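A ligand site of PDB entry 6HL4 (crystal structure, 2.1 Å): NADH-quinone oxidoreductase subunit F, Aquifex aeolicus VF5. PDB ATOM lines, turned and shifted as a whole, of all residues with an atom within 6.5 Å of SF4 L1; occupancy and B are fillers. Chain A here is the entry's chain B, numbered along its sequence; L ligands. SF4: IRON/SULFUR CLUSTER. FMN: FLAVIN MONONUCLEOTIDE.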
ATOM      1  N   ILE A 181      16.149 -19.727   6.727  1.00  0.00           N
ATOM      2  CA  ILE A 181      15.176 -19.457   5.678  1.00  0.00           C
ATOM      3  C   ILE A 181      14.995 -17.938   5.405  1.00  0.00           C
ATOM      4  O   ILE A 181      14.690 -17.580   4.273  1.00  0.00           O
ATOM      5  CB  ILE A 181      13.833 -20.187   5.941  1.00  0.00           C
ATOM      6  CG1 ILE A 181      12.963 -20.316   4.666  1.00  0.00           C
ATOM      7  CG2 ILE A 181      13.019 -19.578   7.113  1.00  0.00           C
ATOM      8  CD1 ILE A 181      13.613 -21.071   3.556  1.00  0.00           C
ATOM      9  N   GLU A 184      16.411 -16.415   2.247  1.00  0.00           N
ATOM     10  CA  GLU A 184      15.641 -16.558   1.025  1.00  0.00           C
ATOM     11  C   GLU A 184      14.956 -15.179   0.840  1.00  0.00           C
ATOM     12  O   GLU A 184      14.358 -14.651   1.801  1.00  0.00           O
ATOM     13  CB  GLU A 184      14.629 -17.720   1.212  1.00  0.00           C
ATOM     14  CG  GLU A 184      14.072 -18.303  -0.065  1.00  0.00           C
ATOM     15  CD  GLU A 184      12.919 -17.554  -0.695  1.00  0.00           C
ATOM     16  OE1 GLU A 184      12.237 -16.758   0.007  1.00  0.00           O
ATOM     17  OE2 GLU A 184      12.690 -17.771  -1.903  1.00  0.00           O
ATOM     18  N   HIS A 198       8.247 -16.866   6.198  1.00  0.00           N
ATOM     19  CA  HIS A 198       7.683 -17.888   5.333  1.00  0.00           C
ATOM     20  C   HIS A 198       7.833 -17.418   3.888  1.00  0.00           C
ATOM     21  O   HIS A 198       7.219 -16.410   3.540  1.00  0.00           O
ATOM     22  CB  HIS A 198       6.193 -18.101   5.655  1.00  0.00           C
ATOM     23  CG  HIS A 198       5.922 -19.094   6.750  1.00  0.00           C
ATOM     24  ND1 HIS A 198       4.627 -19.416   7.120  1.00  0.00           N
ATOM     25  CD2 HIS A 198       6.783 -19.814   7.510  1.00  0.00           C
ATOM     26  CE1 HIS A 198       4.751 -20.309   8.084  1.00  0.00           C
ATOM     27  NE2 HIS A 198       6.025 -20.583   8.357  1.00  0.00           N
ATOM     28  N   PRO A 199       8.624 -18.117   3.037  1.00  0.00           N
ATOM     29  CA  PRO A 199       8.727 -17.700   1.628  1.00  0.00           C
ATOM     30  C   PRO A 199       7.385 -17.690   0.905  1.00  0.00           C
ATOM     31  O   PRO A 199       6.525 -18.552   1.125  1.00  0.00           O
ATOM     32  CB  PRO A 199       9.654 -18.737   1.011  1.00  0.00           C
ATOM     33  CG  PRO A 199      10.402 -19.322   2.144  1.00  0.00           C
ATOM     34  CD  PRO A 199       9.439 -19.316   3.295  1.00  0.00           C
ATOM     35  N   LYS A 202       6.472 -17.960  -5.856  1.00  0.00           N
ATOM     36  CA  LYS A 202       6.982 -17.154  -6.988  1.00  0.00           C
ATOM     37  C   LYS A 202       6.562 -17.823  -8.309  1.00  0.00           C
ATOM     38  O   LYS A 202       6.707 -19.045  -8.428  1.00  0.00           O
ATOM     39  CB  LYS A 202       8.492 -17.003  -6.951  1.00  0.00           C
ATOM     40  CG  LYS A 202       9.093 -16.660  -5.596  1.00  0.00           C
ATOM     41  CD  LYS A 202       9.733 -17.893  -4.992  1.00  0.00           C
ATOM     42  CE  LYS A 202      10.436 -17.557  -3.719  1.00  0.00           C
ATOM     43  NZ  LYS A 202      10.052 -18.465  -2.608  1.00  0.00           N
ATOM     44  N   GLU A 345      16.243 -26.215   9.676  1.00  0.00           N
ATOM     45  CA  GLU A 345      15.949 -24.967   8.960  1.00  0.00           C
ATOM     46  C   GLU A 345      14.717 -24.963   8.035  1.00  0.00           C
ATOM     47  O   GLU A 345      14.316 -23.891   7.605  1.00  0.00           O
ATOM     48  CB  GLU A 345      17.184 -24.482   8.189  1.00  0.00           C
ATOM     49  CG  GLU A 345      18.388 -24.182   9.089  1.00  0.00           C
ATOM     50  CD  GLU A 345      18.238 -23.289  10.316  1.00  0.00           C
ATOM     51  OE1 GLU A 345      17.271 -22.506  10.391  1.00  0.00           O
ATOM     52  OE2 GLU A 345      19.122 -23.364  11.189  1.00  0.00           O
ATOM     53  N   THR A 346      14.101 -26.123   7.750  1.00  0.00           N
ATOM     54  CA  THR A 346      12.888 -26.157   6.925  1.00  0.00           C
ATOM     55  C   THR A 346      11.789 -25.353   7.637  1.00  0.00           C
ATOM     56  O   THR A 346      11.589 -25.549   8.845  1.00  0.00           O
ATOM     57  CB  THR A 346      12.482 -27.605   6.538  1.00  0.00           C
ATOM     58  OG1 THR A 346      11.288 -27.561   5.762  1.00  0.00           O
ATOM     59  CG2 THR A 346      12.293 -28.519   7.750  1.00  0.00           C
ATOM     60  N   CYS A 347      11.156 -24.385   6.927  1.00  0.00           N
ATOM     61  CA  CYS A 347      10.117 -23.549   7.537  1.00  0.00           C
ATOM     62  C   CYS A 347       8.824 -24.315   7.760  1.00  0.00           C
ATOM     63  O   CYS A 347       7.984 -23.872   8.550  1.00  0.00           O
ATOM     64  CB  CYS A 347       9.903 -22.261   6.740  1.00  0.00           C
ATOM     65  SG  CYS A 347       8.852 -22.456   5.286  1.00  0.00           S
ATOM     66  N   GLY A 348       8.688 -25.454   7.080  1.00  0.00           N
ATOM     67  CA  GLY A 348       7.578 -26.384   7.217  1.00  0.00           C
ATOM     68  C   GLY A 348       6.334 -26.091   6.413  1.00  0.00           C
ATOM     69  O   GLY A 348       5.317 -26.742   6.623  1.00  0.00           O
ATOM     70  N   GLN A 349       6.389 -25.101   5.501  1.00  0.00           N
ATOM     71  CA  GLN A 349       5.248 -24.714   4.660  1.00  0.00           C
ATOM     72  C   GLN A 349       4.846 -25.809   3.681  1.00  0.00           C
ATOM     73  O   GLN A 349       3.666 -26.027   3.452  1.00  0.00           O
ATOM     74  CB  GLN A 349       5.556 -23.438   3.875  1.00  0.00           C
ATOM     75  CG  GLN A 349       5.103 -22.179   4.570  1.00  0.00           C
ATOM     76  CD  GLN A 349       5.178 -21.000   3.636  1.00  0.00           C
ATOM     77  OE1 GLN A 349       6.224 -20.723   3.016  1.00  0.00           O
ATOM     78  NE2 GLN A 349       4.075 -20.278   3.516  1.00  0.00           N
ATOM     79  N   CYS A 350       5.832 -26.457   3.063  1.00  0.00           N
ATOM     80  CA  CYS A 350       5.671 -27.523   2.082  1.00  0.00           C
ATOM     81  C   CYS A 350       5.864 -28.854   2.823  1.00  0.00           C
ATOM     82  O   CYS A 350       6.815 -29.008   3.584  1.00  0.00           O
ATOM     83  CB  CYS A 350       6.675 -27.366   0.948  1.00  0.00           C
ATOM     84  SG  CYS A 350       6.926 -25.650   0.417  1.00  0.00           S
ATOM     85  N   THR A 351       4.953 -29.784   2.612  1.00  0.00           N
ATOM     86  CA  THR A 351       4.930 -31.097   3.258  1.00  0.00           C
ATOM     87  C   THR A 351       6.162 -31.948   2.873  1.00  0.00           C
ATOM     88  O   THR A 351       6.883 -32.320   3.813  1.00  0.00           O
ATOM     89  CB  THR A 351       3.577 -31.771   3.000  1.00  0.00           C
ATOM     90  OG1 THR A 351       2.582 -30.991   3.665  1.00  0.00           O
ATOM     91  CG2 THR A 351       3.525 -33.218   3.503  1.00  0.00           C
ATOM     92  N   CYS A 353       9.072 -31.120   2.000  1.00  0.00           N
ATOM     93  CA  CYS A 353      10.231 -30.473   2.580  1.00  0.00           C
ATOM     94  C   CYS A 353      10.186 -30.628   4.101  1.00  0.00           C
ATOM     95  O   CYS A 353      11.190 -31.028   4.687  1.00  0.00           O
ATOM     96  CB  CYS A 353      10.318 -29.001   2.178  1.00  0.00           C
ATOM     97  SG  CYS A 353      11.787 -28.148   2.802  1.00  0.00           S
ATOM     98  N   ARG A 354       9.029 -30.337   4.724  1.00  0.00           N
ATOM     99  CA  ARG A 354       8.830 -30.472   6.176  1.00  0.00           C
ATOM    100  C   ARG A 354       9.166 -31.908   6.623  1.00  0.00           C
ATOM    101  O   ARG A 354      10.040 -32.088   7.463  1.00  0.00           O
ATOM    102  CB  ARG A 354       7.390 -30.096   6.563  1.00  0.00           C
ATOM    103  CG  ARG A 354       7.095 -30.202   8.062  1.00  0.00           C
ATOM    104  CD  ARG A 354       5.678 -29.806   8.458  1.00  0.00           C
ATOM    105  NE  ARG A 354       4.643 -30.120   7.454  1.00  0.00           N
ATOM    106  CZ  ARG A 354       3.969 -31.262   7.365  1.00  0.00           C
ATOM    107  NH1 ARG A 354       4.179 -32.241   8.239  1.00  0.00           N
ATOM    108  NH2 ARG A 354       3.062 -31.427   6.419  1.00  0.00           N
ATOM    109  N   CYS A 357      13.053 -33.276   5.096  1.00  0.00           N
ATOM    110  CA  CYS A 357      14.205 -32.828   5.874  1.00  0.00           C
ATOM    111  C   CYS A 357      14.257 -33.539   7.227  1.00  0.00           C
ATOM    112  O   CYS A 357      15.333 -33.890   7.688  1.00  0.00           O
ATOM    113  CB  CYS A 357      14.193 -31.313   6.046  1.00  0.00           C
ATOM    114  SG  CYS A 357      14.394 -30.380   4.515  1.00  0.00           S
ATOM    115  N   ILE A 387      12.397 -34.680  -1.360  1.00  0.00           N
ATOM    116  CA  ILE A 387      12.248 -33.487  -0.522  1.00  0.00           C
ATOM    117  C   ILE A 387      11.756 -32.333  -1.425  1.00  0.00           C
ATOM    118  O   ILE A 387      10.914 -31.535  -1.003  1.00  0.00           O
ATOM    119  CB  ILE A 387      13.543 -33.148   0.257  1.00  0.00           C
ATOM    120  CG1 ILE A 387      14.025 -34.341   1.134  1.00  0.00           C
ATOM    121  CG2 ILE A 387      13.374 -31.877   1.110  1.00  0.00           C
ATOM    122  CD1 ILE A 387      15.513 -34.259   1.580  1.00  0.00           C
ATOM    123  N   THR A 390       6.704 -30.075  -4.765  1.00  0.00           N
ATOM    124  CA  THR A 390       5.795 -28.987  -4.360  1.00  0.00           C
ATOM    125  C   THR A 390       6.479 -27.844  -3.576  1.00  0.00           C
ATOM    126  O   THR A 390       5.797 -26.893  -3.176  1.00  0.00           O
ATOM    127  CB  THR A 390       4.557 -29.501  -3.594  1.00  0.00           C
ATOM    128  OG1 THR A 390       4.909 -29.726  -2.226  1.00  0.00           O
ATOM    129  CG2 THR A 390       3.913 -30.742  -4.225  1.00  0.00           C
ATOM    130  N   SER A 391       7.813 -27.933  -3.360  1.00  0.00           N
ATOM    131  CA  SER A 391       8.562 -26.913  -2.651  1.00  0.00           C
ATOM    132  C   SER A 391       8.395 -25.548  -3.334  1.00  0.00           C
ATOM    133  O   SER A 391       8.444 -25.469  -4.556  1.00  0.00           O
ATOM    134  CB  SER A 391      10.037 -27.298  -2.563  1.00  0.00           C
ATOM    135  OG  SER A 391      10.618 -27.383  -3.848  1.00  0.00           O
ATOM    136  N   ILE A 392       8.160 -24.493  -2.531  1.00  0.00           N
ATOM    137  CA  ILE A 392       7.979 -23.137  -3.051  1.00  0.00           C
ATOM    138  C   ILE A 392       9.231 -22.263  -2.869  1.00  0.00           C
ATOM    139  O   ILE A 392       9.192 -21.071  -3.194  1.00  0.00           O
ATOM    140  CB  ILE A 392       6.685 -22.432  -2.555  1.00  0.00           C
ATOM    141  CG1 ILE A 392       6.552 -22.469  -1.012  1.00  0.00           C
ATOM    142  CG2 ILE A 392       5.456 -23.008  -3.256  1.00  0.00           C
ATOM    143  CD1 ILE A 392       5.537 -21.463  -0.408  1.00  0.00           C
ATOM    144  N   CYS A 393      10.338 -22.856  -2.393  1.00  0.00           N
ATOM    145  CA  CYS A 393      11.614 -22.152  -2.250  1.00  0.00           C
ATOM    146  C   CYS A 393      12.808 -23.094  -2.470  1.00  0.00           C
ATOM    147  O   CYS A 393      12.633 -24.302  -2.541  1.00  0.00           O
ATOM    148  CB  CYS A 393      11.715 -21.390  -0.926  1.00  0.00           C
ATOM    149  SG  CYS A 393      12.652 -22.254   0.366  1.00  0.00           S
ATOM    150  N   GLY A 394      13.994 -22.516  -2.610  1.00  0.00           N
ATOM    151  CA  GLY A 394      15.234 -23.222  -2.897  1.00  0.00           C
ATOM    152  C   GLY A 394      15.716 -24.257  -1.894  1.00  0.00           C
ATOM    153  O   GLY A 394      16.461 -25.159  -2.286  1.00  0.00           O
ATOM    154  N   LEU A 395      15.309 -24.155  -0.605  1.00  0.00           N
ATOM    155  CA  LEU A 395      15.731 -25.093   0.456  1.00  0.00           C
ATOM    156  C   LEU A 395      15.299 -26.520   0.134  1.00  0.00           C
ATOM    157  O   LEU A 395      16.134 -27.436   0.181  1.00  0.00           O
ATOM    158  CB  LEU A 395      15.215 -24.655   1.839  1.00  0.00           C
ATOM    159  CG  LEU A 395      15.821 -25.363   3.062  1.00  0.00           C
ATOM    160  CD1 LEU A 395      15.906 -24.451   4.267  1.00  0.00           C
ATOM    161  CD2 LEU A 395      15.044 -26.598   3.427  1.00  0.00           C
ATOM    162  N   GLY A 396      14.018 -26.691  -0.215  1.00  0.00           N
ATOM    163  CA  GLY A 396      13.423 -27.969  -0.579  1.00  0.00           C
ATOM    164  C   GLY A 396      14.093 -28.604  -1.780  1.00  0.00           C
ATOM    165  O   GLY A 396      14.321 -29.814  -1.791  1.00  0.00           O
ATOM    166  N   ALA A 397      14.467 -27.778  -2.775  1.00  0.00           N
ATOM    167  CA  ALA A 397      15.131 -28.256  -3.994  1.00  0.00           C
ATOM    168  C   ALA A 397      16.561 -28.759  -3.778  1.00  0.00           C
ATOM    169  O   ALA A 397      17.031 -29.593  -4.556  1.00  0.00           O
ATOM    170  CB  ALA A 397      15.145 -27.150  -5.033  1.00  0.00           C
HETATM  171 FE1  SF4 L   1       9.718 -23.773   3.724  1.00  0.00          FE
HETATM  172 FE2  SF4 L   1      10.989 -25.961   2.669  1.00  0.00          FE
HETATM  173 FE3  SF4 L   1      11.103 -23.545   1.360  1.00  0.00          FE
HETATM  174 FE4  SF4 L   1       8.782 -24.966   1.395  1.00  0.00          FE
HETATM  175  S1  SF4 L   1      10.721 -25.588   0.406  1.00  0.00           S
HETATM  176  S2  SF4 L   1       9.015 -22.717   1.778  1.00  0.00           S
HETATM  177  S3  SF4 L   1       8.877 -25.901   3.515  1.00  0.00           S
HETATM  178  S4  SF4 L   1      11.957 -24.044   3.447  1.00  0.00           S
HETATM  179  N1  FMN L   2      21.397 -14.927  -0.163  1.00  0.00           N
HETATM  180  C2  FMN L   2      22.150 -14.143   0.660  1.00  0.00           C
HETATM  181  O2  FMN L   2      22.565 -13.043   0.283  1.00  0.00           O
HETATM  182  N3  FMN L   2      22.343 -14.509   1.997  1.00  0.00           N
HETATM  183  C4  FMN L   2      21.784 -15.604   2.624  1.00  0.00           C
HETATM  184  O4  FMN L   2      21.960 -15.787   3.825  1.00  0.00           O
HETATM  185  C4A FMN L   2      20.953 -16.422   1.749  1.00  0.00           C
HETATM  186  N5  FMN L   2      20.316 -17.435   2.272  1.00  0.00           N
HETATM  187  C5A FMN L   2      19.429 -18.139   1.463  1.00  0.00           C
HETATM  188  C6  FMN L   2      18.689 -19.180   2.033  1.00  0.00           C
HETATM  189  C7  FMN L   2      17.796 -19.924   1.281  1.00  0.00           C
HETATM  190  C7M FMN L   2      17.008 -21.030   1.949  1.00  0.00           C
HETATM  191  C8  FMN L   2      17.634 -19.636  -0.100  1.00  0.00           C
HETATM  192  C8M FMN L   2      16.792 -20.505  -0.998  1.00  0.00           C
HETATM  193  C9  FMN L   2      18.346 -18.573  -0.656  1.00  0.00           C
HETATM  194  C9A FMN L   2      19.226 -17.812   0.102  1.00  0.00           C
HETATM  195  N10 FMN L   2      19.927 -16.701  -0.433  1.00  0.00           N
HETATM  196  C10 FMN L   2      20.810 -15.991   0.364  1.00  0.00           C
HETATM  197  C1' FMN L   2      19.676 -16.276  -1.816  1.00  0.00           C
HETATM  198  C2' FMN L   2      18.622 -15.185  -1.936  1.00  0.00           C
HETATM  199  O2' FMN L   2      17.327 -15.782  -2.109  1.00  0.00           O
HETATM  200  C3' FMN L   2      18.895 -14.248  -3.103  1.00  0.00           C
HETATM  201  O3' FMN L   2      19.122 -15.007  -4.284  1.00  0.00           O
HETATM  202  C4' FMN L   2      20.051 -13.247  -2.942  1.00  0.00           C
HETATM  203  O4' FMN L   2      19.970 -12.530  -1.709  1.00  0.00           O
HETATM  204  C5' FMN L   2      20.097 -12.273  -4.097  1.00  0.00           C
HETATM  205  O5' FMN L   2      21.264 -11.439  -3.968  1.00  0.00           O
HETATM  206  P   FMN L   2      22.466 -11.577  -5.041  1.00  0.00           P
HETATM  207  O1P FMN L   2      23.162 -12.871  -4.859  1.00  0.00           O
HETATM  208  O2P FMN L   2      21.889 -11.402  -6.443  1.00  0.00           O
HETATM  209  O3P FMN L   2      23.345 -10.382  -4.747  1.00  0.00           O
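Ile 181 touches SF4 L1 (CD1 to S4, 3.4 Å).
Pro 199 touches SF4 L1.
Ser 391 touches SF4 L1 (CB to S1, 3.5 Å).
CG1 of Ile 392 touches S2 of SF4 L1 (3.7 Å).
CB of Leu 395 touches S4 of SF4 L1, 3.7 Å away.
13 residues have an atom within 4 Å of SF4 L1: Ile 181, Pro 199, Thr 346, Cys 347, Gly 348, Gln 349, Cys 350, Cys 353, Ser 391, Ile 392, Cys 393, Leu 395 and Gly 396.
The nearest printed residue that does not touch SF4 L1 is Arg 354 (4.6 Å).
The side-chain sulfur (SG) of Cys 350 is bound to an iron atom (FE4) of SF4 L1, at 2.2 Å.
The side-chain sulfur (SG) of Cys 347 is bound to an iron atom (FE1) of SF4 L1 (2.2 Å).
The backbone NH (N) of Cys 347 lies close to a sulfur (S4) of SF4 L1, at 3.6 Å.
The side-chain amide oxygen of Gln 349 sits close to a sulfur (S2) of SF4 L1 (3.6 Å).
A sulfur (S1) of SF4 L1 lies close to the backbone NH (N) of Gly 396.
The backbone NH (N) of Cys 350 sits close to a sulfur (S3) of SF4 L1, at 3.1 Å.
An iron atom (FE2) of SF4 L1 is bound by the side-chain sulfur of Cys 353 (2.3 Å).
N of Gln 349 lies close to S3 of SF4 L1 (3.3 Å).
N of Gly 348 lies close to S3 of SF4 L1, at 3.6 Å.
An iron atom (FE3) of SF4 L1 is bound by the side-chain sulfur (SG) of Cys 393, at 2.2 Å.
A sulfur (S3) of SF4 L1 sits close to the side-chain hydroxyl of Thr 346 (3.7 Å).
OE1 of Gln 349 lies close to O of Pro 199 (2.9 Å).
The side-chain sulfur of Cys 393 sits close to the backbone NH of Leu 395, at 3.4 Å.
The backbone NH (N) of Gln 349 lies close to the side-chain sulfur (SG) of Cys 347.
O of Ile 392 sits at hydrogen-bond distance from NZ of Lys 202 (2.8 Å).
SG of Cys 357 lies within hydrogen-bond range of O of Cys 353 (3.3 Å).
The backbone NH of Ile 392 lies close to the side-chain sulfur of Cys 350, at 3.4 Å.
The side-chain sulfur (SG) of Cys 353 sits close to the side-chain hydroxyl (OG1) of Thr 346.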
